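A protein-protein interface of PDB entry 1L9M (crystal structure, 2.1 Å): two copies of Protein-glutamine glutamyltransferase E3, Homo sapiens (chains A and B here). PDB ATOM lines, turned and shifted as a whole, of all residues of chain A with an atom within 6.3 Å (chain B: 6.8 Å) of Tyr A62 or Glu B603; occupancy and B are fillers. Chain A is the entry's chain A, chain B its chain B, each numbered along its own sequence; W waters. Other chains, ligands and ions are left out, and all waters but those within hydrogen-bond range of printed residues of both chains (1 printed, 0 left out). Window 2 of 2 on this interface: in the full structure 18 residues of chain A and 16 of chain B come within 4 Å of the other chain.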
ATOM      1  N   THR A  59     -12.465 -28.829   9.305  1.00  0.00           N
ATOM      2  CA  THR A  59     -12.763 -30.156   8.782  1.00  0.00           C
ATOM      3  C   THR A  59     -11.954 -30.417   7.512  1.00  0.00           C
ATOM      4  O   THR A  59     -11.651 -29.490   6.756  1.00  0.00           O
ATOM      5  CB  THR A  59     -14.290 -30.315   8.492  1.00  0.00           C
ATOM      6  OG1 THR A  59     -14.545 -31.627   7.974  1.00  0.00           O
ATOM      7  CG2 THR A  59     -14.766 -29.276   7.493  1.00  0.00           C
ATOM      8  N   GLY A  60     -11.587 -31.674   7.289  1.00  0.00           N
ATOM      9  CA  GLY A  60     -10.814 -32.009   6.103  1.00  0.00           C
ATOM     10  C   GLY A  60      -9.310 -31.846   6.274  1.00  0.00           C
ATOM     11  O   GLY A  60      -8.849 -31.307   7.284  1.00  0.00           O
ATOM     12  N   PRO A  61      -8.513 -32.302   5.297  1.00  0.00           N
ATOM     13  CA  PRO A  61      -7.049 -32.205   5.348  1.00  0.00           C
ATOM     14  C   PRO A  61      -6.435 -30.831   5.049  1.00  0.00           C
ATOM     15  O   PRO A  61      -5.233 -30.639   5.235  1.00  0.00           O
ATOM     16  CB  PRO A  61      -6.604 -33.257   4.337  1.00  0.00           C
ATOM     17  CG  PRO A  61      -7.682 -33.181   3.305  1.00  0.00           C
ATOM     18  CD  PRO A  61      -8.940 -33.126   4.150  1.00  0.00           C
ATOM     19  N   TYR A  62      -7.246 -29.884   4.589  1.00  0.00           N
ATOM     20  CA  TYR A  62      -6.743 -28.547   4.262  1.00  0.00           C
ATOM     21  C   TYR A  62      -7.715 -27.464   4.726  1.00  0.00           C
ATOM     22  O   TYR A  62      -8.222 -26.685   3.915  1.00  0.00           O
ATOM     23  CB  TYR A  62      -6.525 -28.433   2.750  1.00  0.00           C
ATOM     24  CG  TYR A  62      -5.593 -29.491   2.195  1.00  0.00           C
ATOM     25  CD1 TYR A  62      -4.219 -29.441   2.442  1.00  0.00           C
ATOM     26  CD2 TYR A  62      -6.087 -30.556   1.443  1.00  0.00           C
ATOM     27  CE1 TYR A  62      -3.359 -30.432   1.948  1.00  0.00           C
ATOM     28  CE2 TYR A  62      -5.239 -31.551   0.945  1.00  0.00           C
ATOM     29  CZ  TYR A  62      -3.877 -31.481   1.200  1.00  0.00           C
ATOM     30  OH  TYR A  62      -3.040 -32.453   0.696  1.00  0.00           O
ATOM     31  N   PRO A  63      -7.980 -27.403   6.045  1.00  0.00           N
ATOM     32  CA  PRO A  63      -8.887 -26.438   6.671  1.00  0.00           C
ATOM     33  C   PRO A  63      -8.593 -25.015   6.223  1.00  0.00           C
ATOM     34  O   PRO A  63      -7.473 -24.525   6.390  1.00  0.00           O
ATOM     35  CB  PRO A  63      -8.613 -26.627   8.163  1.00  0.00           C
ATOM     36  CG  PRO A  63      -8.230 -28.049   8.257  1.00  0.00           C
ATOM     37  CD  PRO A  63      -7.326 -28.232   7.072  1.00  0.00           C
ATOM     38  N   SER A  64      -9.599 -24.351   5.669  1.00  0.00           N
ATOM     39  CA  SER A  64      -9.431 -22.982   5.200  1.00  0.00           C
ATOM     40  C   SER A  64     -10.670 -22.125   5.436  1.00  0.00           C
ATOM     41  O   SER A  64     -11.799 -22.544   5.148  1.00  0.00           O
ATOM     42  CB  SER A  64      -9.093 -22.983   3.708  1.00  0.00           C
ATOM     43  OG  SER A  64      -9.064 -21.664   3.200  1.00  0.00           O
ATOM     44  N   ALA A  67     -12.583 -21.356   2.312  1.00  0.00           N
ATOM     45  CA  ALA A  67     -13.328 -22.493   1.781  1.00  0.00           C
ATOM     46  C   ALA A  67     -14.458 -22.913   2.717  1.00  0.00           C
ATOM     47  O   ALA A  67     -15.141 -23.905   2.466  1.00  0.00           O
ATOM     48  CB  ALA A  67     -12.388 -23.666   1.549  1.00  0.00           C
ATOM     49  N   THR A  69     -14.224 -24.361   5.275  1.00  0.00           N
ATOM     50  CA  THR A  69     -13.868 -25.611   5.940  1.00  0.00           C
ATOM     51  C   THR A  69     -13.116 -25.348   7.242  1.00  0.00           C
ATOM     52  O   THR A  69     -12.584 -26.269   7.862  1.00  0.00           O
ATOM     53  CB  THR A  69     -13.016 -26.544   5.034  1.00  0.00           C
ATOM     54  OG1 THR A  69     -11.890 -25.828   4.515  1.00  0.00           O
ATOM     55  CG2 THR A  69     -13.862 -27.082   3.882  1.00  0.00           C
ATOM     56  N   ARG A 199      -9.861 -37.580  -4.083  1.00  0.00           N
ATOM     57  CA  ARG A 199      -8.498 -37.879  -4.521  1.00  0.00           C
ATOM     58  C   ARG A 199      -7.993 -36.814  -5.495  1.00  0.00           C
ATOM     59  O   ARG A 199      -6.820 -36.464  -5.501  1.00  0.00           O
ATOM     60  CB  ARG A 199      -8.440 -39.246  -5.211  1.00  0.00           C
ATOM     61  CG  ARG A 199      -8.963 -40.403  -4.374  1.00  0.00           C
ATOM     62  CD  ARG A 199      -8.676 -41.749  -5.036  1.00  0.00           C
ATOM     63  NE  ARG A 199      -9.320 -42.857  -4.332  1.00  0.00           N
ATOM     64  CZ  ARG A 199      -9.195 -43.101  -3.026  1.00  0.00           C
ATOM     65  NH1 ARG A 199      -8.445 -42.314  -2.258  1.00  0.00           N
ATOM     66  NH2 ARG A 199      -9.828 -44.134  -2.481  1.00  0.00           N
ATOM     67  N   ARG A 200      -8.895 -36.302  -6.318  1.00  0.00           N
ATOM     68  CA  ARG A 200      -8.541 -35.290  -7.302  1.00  0.00           C
ATOM     69  C   ARG A 200      -8.205 -33.944  -6.652  1.00  0.00           C
ATOM     70  O   ARG A 200      -7.270 -33.259  -7.069  1.00  0.00           O
ATOM     71  CB  ARG A 200      -9.707 -35.123  -8.276  1.00  0.00           C
ATOM     72  CG  ARG A 200      -9.327 -34.823  -9.714  1.00  0.00           C
ATOM     73  CD  ARG A 200     -10.324 -35.500 -10.650  1.00  0.00           C
ATOM     74  NE  ARG A 200     -11.706 -35.207 -10.271  1.00  0.00           N
ATOM     75  CZ  ARG A 200     -12.667 -36.123 -10.159  1.00  0.00           C
ATOM     76  NH1 ARG A 200     -12.410 -37.404 -10.395  1.00  0.00           N
ATOM     77  NH2 ARG A 200     -13.891 -35.757  -9.806  1.00  0.00           N
ATOM     78  N   ASP A 201      -8.966 -33.573  -5.627  1.00  0.00           N
ATOM     79  CA  ASP A 201      -8.764 -32.299  -4.941  1.00  0.00           C
ATOM     80  C   ASP A 201      -9.478 -32.358  -3.588  1.00  0.00           C
ATOM     81  O   ASP A 201     -10.644 -31.986  -3.478  1.00  0.00           O
ATOM     82  CB  ASP A 201      -9.352 -31.169  -5.797  1.00  0.00           C
ATOM     83  CG  ASP A 201      -9.102 -29.779  -5.216  1.00  0.00           C
ATOM     84  OD1 ASP A 201      -9.001 -29.626  -3.979  1.00  0.00           O
ATOM     85  OD2 ASP A 201      -9.029 -28.823  -6.011  1.00  0.00           O
ATOM     86  N   ALA A 202      -8.776 -32.824  -2.562  1.00  0.00           N
ATOM     87  CA  ALA A 202      -9.363 -32.937  -1.237  1.00  0.00           C
ATOM     88  C   ALA A 202      -9.940 -31.623  -0.726  1.00  0.00           C
ATOM     89  O   ALA A 202     -11.060 -31.593  -0.209  1.00  0.00           O
ATOM     90  CB  ALA A 202      -8.331 -33.463  -0.260  1.00  0.00           C
ATOM     91  N   ALA A 203      -9.186 -30.538  -0.875  1.00  0.00           N
ATOM     92  CA  ALA A 203      -9.629 -29.230  -0.394  1.00  0.00           C
ATOM     93  C   ALA A 203     -10.979 -28.813  -0.959  1.00  0.00           C
ATOM     94  O   ALA A 203     -11.877 -28.401  -0.218  1.00  0.00           O
ATOM     95  CB  ALA A 203      -8.577 -28.164  -0.713  1.00  0.00           C
ATOM     96  N   VAL B 600       0.016 -25.075   3.664  1.00  0.00           N
ATOM     97  CA  VAL B 600      -0.245 -25.301   2.254  1.00  0.00           C
ATOM     98  C   VAL B 600      -1.680 -25.839   2.232  1.00  0.00           C
ATOM     99  O   VAL B 600      -2.025 -26.711   3.031  1.00  0.00           O
ATOM    100  CB  VAL B 600       0.721 -26.343   1.656  1.00  0.00           C
ATOM    101  CG1 VAL B 600       0.456 -26.498   0.170  1.00  0.00           C
ATOM    102  CG2 VAL B 600       2.158 -25.905   1.877  1.00  0.00           C
ATOM    103  N   LEU B 601      -2.517 -25.311   1.345  1.00  0.00           N
ATOM    104  CA  LEU B 601      -3.910 -25.745   1.272  1.00  0.00           C
ATOM    105  C   LEU B 601      -4.224 -26.810   0.228  1.00  0.00           C
ATOM    106  O   LEU B 601      -5.347 -26.896  -0.267  1.00  0.00           O
ATOM    107  CB  LEU B 601      -4.818 -24.529   1.069  1.00  0.00           C
ATOM    108  CG  LEU B 601      -5.226 -23.757   2.329  1.00  0.00           C
ATOM    109  CD1 LEU B 601      -4.437 -24.236   3.537  1.00  0.00           C
ATOM    110  CD2 LEU B 601      -5.026 -22.280   2.096  1.00  0.00           C
ATOM    111  N   ASN B 602      -3.230 -27.625  -0.098  1.00  0.00           N
ATOM    112  CA  ASN B 602      -3.409 -28.703  -1.062  1.00  0.00           C
ATOM    113  C   ASN B 602      -2.108 -29.453  -1.286  1.00  0.00           C
ATOM    114  O   ASN B 602      -1.062 -29.109  -0.733  1.00  0.00           O
ATOM    115  CB  ASN B 602      -3.911 -28.166  -2.412  1.00  0.00           C
ATOM    116  CG  ASN B 602      -4.727 -29.202  -3.190  1.00  0.00           C
ATOM    117  OD1 ASN B 602      -4.235 -30.284  -3.523  1.00  0.00           O
ATOM    118  ND2 ASN B 602      -5.987 -28.868  -3.476  1.00  0.00           N
ATOM    119  N   GLU B 603      -2.200 -30.489  -2.102  1.00  0.00           N
ATOM    120  CA  GLU B 603      -1.070 -31.323  -2.467  1.00  0.00           C
ATOM    121  C   GLU B 603      -0.076 -30.427  -3.206  1.00  0.00           C
ATOM    122  O   GLU B 603      -0.473 -29.441  -3.825  1.00  0.00           O
ATOM    123  CB  GLU B 603      -1.582 -32.422  -3.392  1.00  0.00           C
ATOM    124  CG  GLU B 603      -0.734 -33.653  -3.500  1.00  0.00           C
ATOM    125  CD  GLU B 603      -1.489 -34.776  -4.184  1.00  0.00           C
ATOM    126  OE1 GLU B 603      -1.801 -34.638  -5.392  1.00  0.00           O
ATOM    127  OE2 GLU B 603      -1.785 -35.786  -3.502  1.00  0.00           O
ATOM    128  N   ALA B 604       1.209 -30.757  -3.141  1.00  0.00           N
ATOM    129  CA  ALA B 604       2.222 -29.960  -3.828  1.00  0.00           C
ATOM    130  C   ALA B 604       2.765 -30.708  -5.042  1.00  0.00           C
ATOM    131  O   ALA B 604       3.423 -31.744  -4.901  1.00  0.00           O
ATOM    132  CB  ALA B 604       3.363 -29.611  -2.870  1.00  0.00           C
ATOM    133  N   ARG B 605       2.491 -30.179  -6.232  1.00  0.00           N
ATOM    134  CA  ARG B 605       2.951 -30.814  -7.459  1.00  0.00           C
ATOM    135  C   ARG B 605       3.652 -29.851  -8.404  1.00  0.00           C
ATOM    136  O   ARG B 605       3.295 -28.674  -8.500  1.00  0.00           O
ATOM    137  CB  ARG B 605       1.776 -31.475  -8.178  1.00  0.00           C
ATOM    138  CG  ARG B 605       0.965 -32.414  -7.290  1.00  0.00           C
ATOM    139  CD  ARG B 605       0.150 -33.366  -8.134  1.00  0.00           C
ATOM    140  NE  ARG B 605       1.023 -34.209  -8.944  1.00  0.00           N
ATOM    141  CZ  ARG B 605       0.627 -34.868 -10.027  1.00  0.00           C
ATOM    142  NH1 ARG B 605      -0.631 -34.783 -10.433  1.00  0.00           N
ATOM    143  NH2 ARG B 605       1.492 -35.611 -10.704  1.00  0.00           N
ATOM    144  N   LYS B 608       2.274 -26.849 -10.821  1.00  0.00           N
ATOM    145  CA  LYS B 608       0.875 -26.626 -10.482  1.00  0.00           C
ATOM    146  C   LYS B 608       0.788 -25.670  -9.298  1.00  0.00           C
ATOM    147  O   LYS B 608       1.291 -25.955  -8.215  1.00  0.00           O
ATOM    148  CB  LYS B 608       0.179 -27.952 -10.143  1.00  0.00           C
ATOM    149  CG  LYS B 608       0.209 -28.955 -11.284  1.00  0.00           C
ATOM    150  CD  LYS B 608      -0.342 -28.334 -12.558  1.00  0.00           C
ATOM    151  CE  LYS B 608       0.001 -29.168 -13.775  1.00  0.00           C
ATOM    152  NZ  LYS B 608      -0.350 -28.440 -15.024  1.00  0.00           N
ATOM    153  N   PRO B 609       0.149 -24.515  -9.497  1.00  0.00           N
ATOM    154  CA  PRO B 609       0.009 -23.525  -8.431  1.00  0.00           C
ATOM    155  C   PRO B 609      -0.749 -24.078  -7.233  1.00  0.00           C
ATOM    156  O   PRO B 609      -1.692 -24.848  -7.394  1.00  0.00           O
ATOM    157  CB  PRO B 609      -0.763 -22.394  -9.110  1.00  0.00           C
ATOM    158  CG  PRO B 609      -0.358 -22.522 -10.545  1.00  0.00           C
ATOM    159  CD  PRO B 609      -0.424 -24.013 -10.755  1.00  0.00           C
ATOM    160  N   VAL B 610      -0.324 -23.699  -6.035  1.00  0.00           N
ATOM    161  CA  VAL B 610      -1.014 -24.134  -4.830  1.00  0.00           C
ATOM    162  C   VAL B 610      -1.108 -22.960  -3.866  1.00  0.00           C
ATOM    163  O   VAL B 610      -0.166 -22.174  -3.738  1.00  0.00           O
ATOM    164  CB  VAL B 610      -0.306 -25.308  -4.133  1.00  0.00           C
ATOM    165  CG1 VAL B 610       1.053 -24.878  -3.611  1.00  0.00           C
ATOM    166  CG2 VAL B 610      -1.194 -25.826  -2.995  1.00  0.00           C
ATOM    167  N   GLN B 613      -1.347 -20.425   3.195  1.00  0.00           N
ATOM    168  CA  GLN B 613      -1.963 -19.571   4.195  1.00  0.00           C
ATOM    169  C   GLN B 613      -0.984 -19.137   5.284  1.00  0.00           C
ATOM    170  O   GLN B 613      -0.263 -19.962   5.850  1.00  0.00           O
ATOM    171  CB  GLN B 613      -3.133 -20.315   4.832  1.00  0.00           C
ATOM    172  CG  GLN B 613      -4.347 -19.464   5.042  1.00  0.00           C
ATOM    173  CD  GLN B 613      -5.572 -20.286   5.380  1.00  0.00           C
ATOM    174  OE1 GLN B 613      -6.700 -19.832   5.186  1.00  0.00           O
ATOM    175  NE2 GLN B 613      -5.360 -21.501   5.892  1.00  0.00           N
ATOM    176  N   PRO B 662       5.507 -24.670  -7.425  1.00  0.00           N
ATOM    177  CA  PRO B 662       6.600 -25.651  -7.400  1.00  0.00           C
ATOM    178  C   PRO B 662       7.228 -25.809  -8.784  1.00  0.00           C
ATOM    179  O   PRO B 662       6.519 -25.925  -9.786  1.00  0.00           O
ATOM    180  CB  PRO B 662       5.908 -26.925  -6.930  1.00  0.00           C
ATOM    181  CG  PRO B 662       4.820 -26.402  -6.037  1.00  0.00           C
ATOM    182  CD  PRO B 662       4.282 -25.229  -6.827  1.00  0.00           C
ATOM    183  N   ILE B 688       7.958 -28.754   2.460  1.00  0.00           N
ATOM    184  CA  ILE B 688       6.917 -29.170   1.533  1.00  0.00           C
ATOM    185  C   ILE B 688       7.418 -30.234   0.570  1.00  0.00           C
ATOM    186  O   ILE B 688       8.476 -30.068  -0.043  1.00  0.00           O
ATOM    187  CB  ILE B 688       6.435 -27.974   0.687  1.00  0.00           C
ATOM    188  CG1 ILE B 688       5.969 -26.835   1.600  1.00  0.00           C
ATOM    189  CG2 ILE B 688       5.340 -28.421  -0.266  1.00  0.00           C
ATOM    190  CD1 ILE B 688       5.521 -25.589   0.854  1.00  0.00           C
ATOM    191  N   ASP B 689       6.662 -31.322   0.425  1.00  0.00           N
ATOM    192  CA  ASP B 689       7.053 -32.379  -0.505  1.00  0.00           C
ATOM    193  C   ASP B 689       6.393 -32.148  -1.857  1.00  0.00           C
ATOM    194  O   ASP B 689       5.174 -32.250  -1.985  1.00  0.00           O
ATOM    195  CB  ASP B 689       6.659 -33.760   0.019  1.00  0.00           C
ATOM    196  CG  ASP B 689       7.464 -34.170   1.227  1.00  0.00           C
ATOM    197  OD1 ASP B 689       8.709 -34.039   1.196  1.00  0.00           O
ATOM    198  OD2 ASP B 689       6.847 -34.628   2.209  1.00  0.00           O
ATOM    199  N   ALA B 691       5.768 -33.327  -5.592  1.00  0.00           N
ATOM    200  CA  ALA B 691       5.771 -34.529  -6.417  1.00  0.00           C
ATOM    201  C   ALA B 691       5.784 -34.114  -7.876  1.00  0.00           C
ATOM    202  O   ALA B 691       5.419 -32.986  -8.212  1.00  0.00           O
ATOM    203  CB  ALA B 691       4.530 -35.384  -6.127  1.00  0.00           C
HETATM  204  O   HOH W   1      -5.585 -31.314  -6.202  1.00  0.00           O
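The side-chain carboxylate (OD1) of Asp A201 is in hydrogen-bond range of the side-chain amide nitrogen (ND2) of Asn B602 (3.1 Å).
OD1 of Asp A201 lies within hydrogen-bond range of N of Ala A203, at 3.2 Å. N of Ser A64 sits at hydrogen-bond distance from OG1 of Thr A69.
Tyr A62 touches Val B600. CD1 of Tyr A62 touches C of Leu B601, 3.4 Å away. Asn B602 touches Tyr A62. Tyr A62 touches Glu B603. NE2 of Gln B613 touches O of Pro A63 (3.7 Å). Gln B613 touches Ser A64. Ala A203 touches Leu B601. CB of Ala A203 touches ND2 of Asn B602 (3.9 Å).
Pro A61 touches none of the printed residues of chain B. Tyr A62 touches just these residues of chain B: Val B600, Leu B601, Asn B602 and Glu B603. Of the printed residues of chain B, Asp A201 touches Asn B602. Of the printed residues of chain B, Ala A203 touches Leu B601 (3.5 Å) and Asn B602 (3.9 Å). Of the printed residues of chain A, Leu B601 touches Tyr A62 and Ala A203. Of chain A, only Tyr A62 comes within 4 Å of Glu B603. Ala B604 touches none of the printed residues of chain A. The nearest residue of chain A that does not touch Glu B603 is Arg A199 (5.3 Å). The nearest printed residue of chain A that does not touch Val B600 is Pro A61 (5.5 Å).
Printed residues of chain B that touch a printed residue of chain A: Val B600, Leu B601, Asn B602, Glu B603 and Gln B613. Among the printed residues, 9 pairs touch across the chains.
No position is printed for both chains. Of the 9 pairs that touch across the chains among the printed residues, none has its exchanged pair printed and touching as well.
Water W1 bridges the backbone carbonyl oxygen (O) of Arg A200 (2.7 Å) and the side-chain amide oxygen (OD1) of Asn B602 (3.2 Å).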
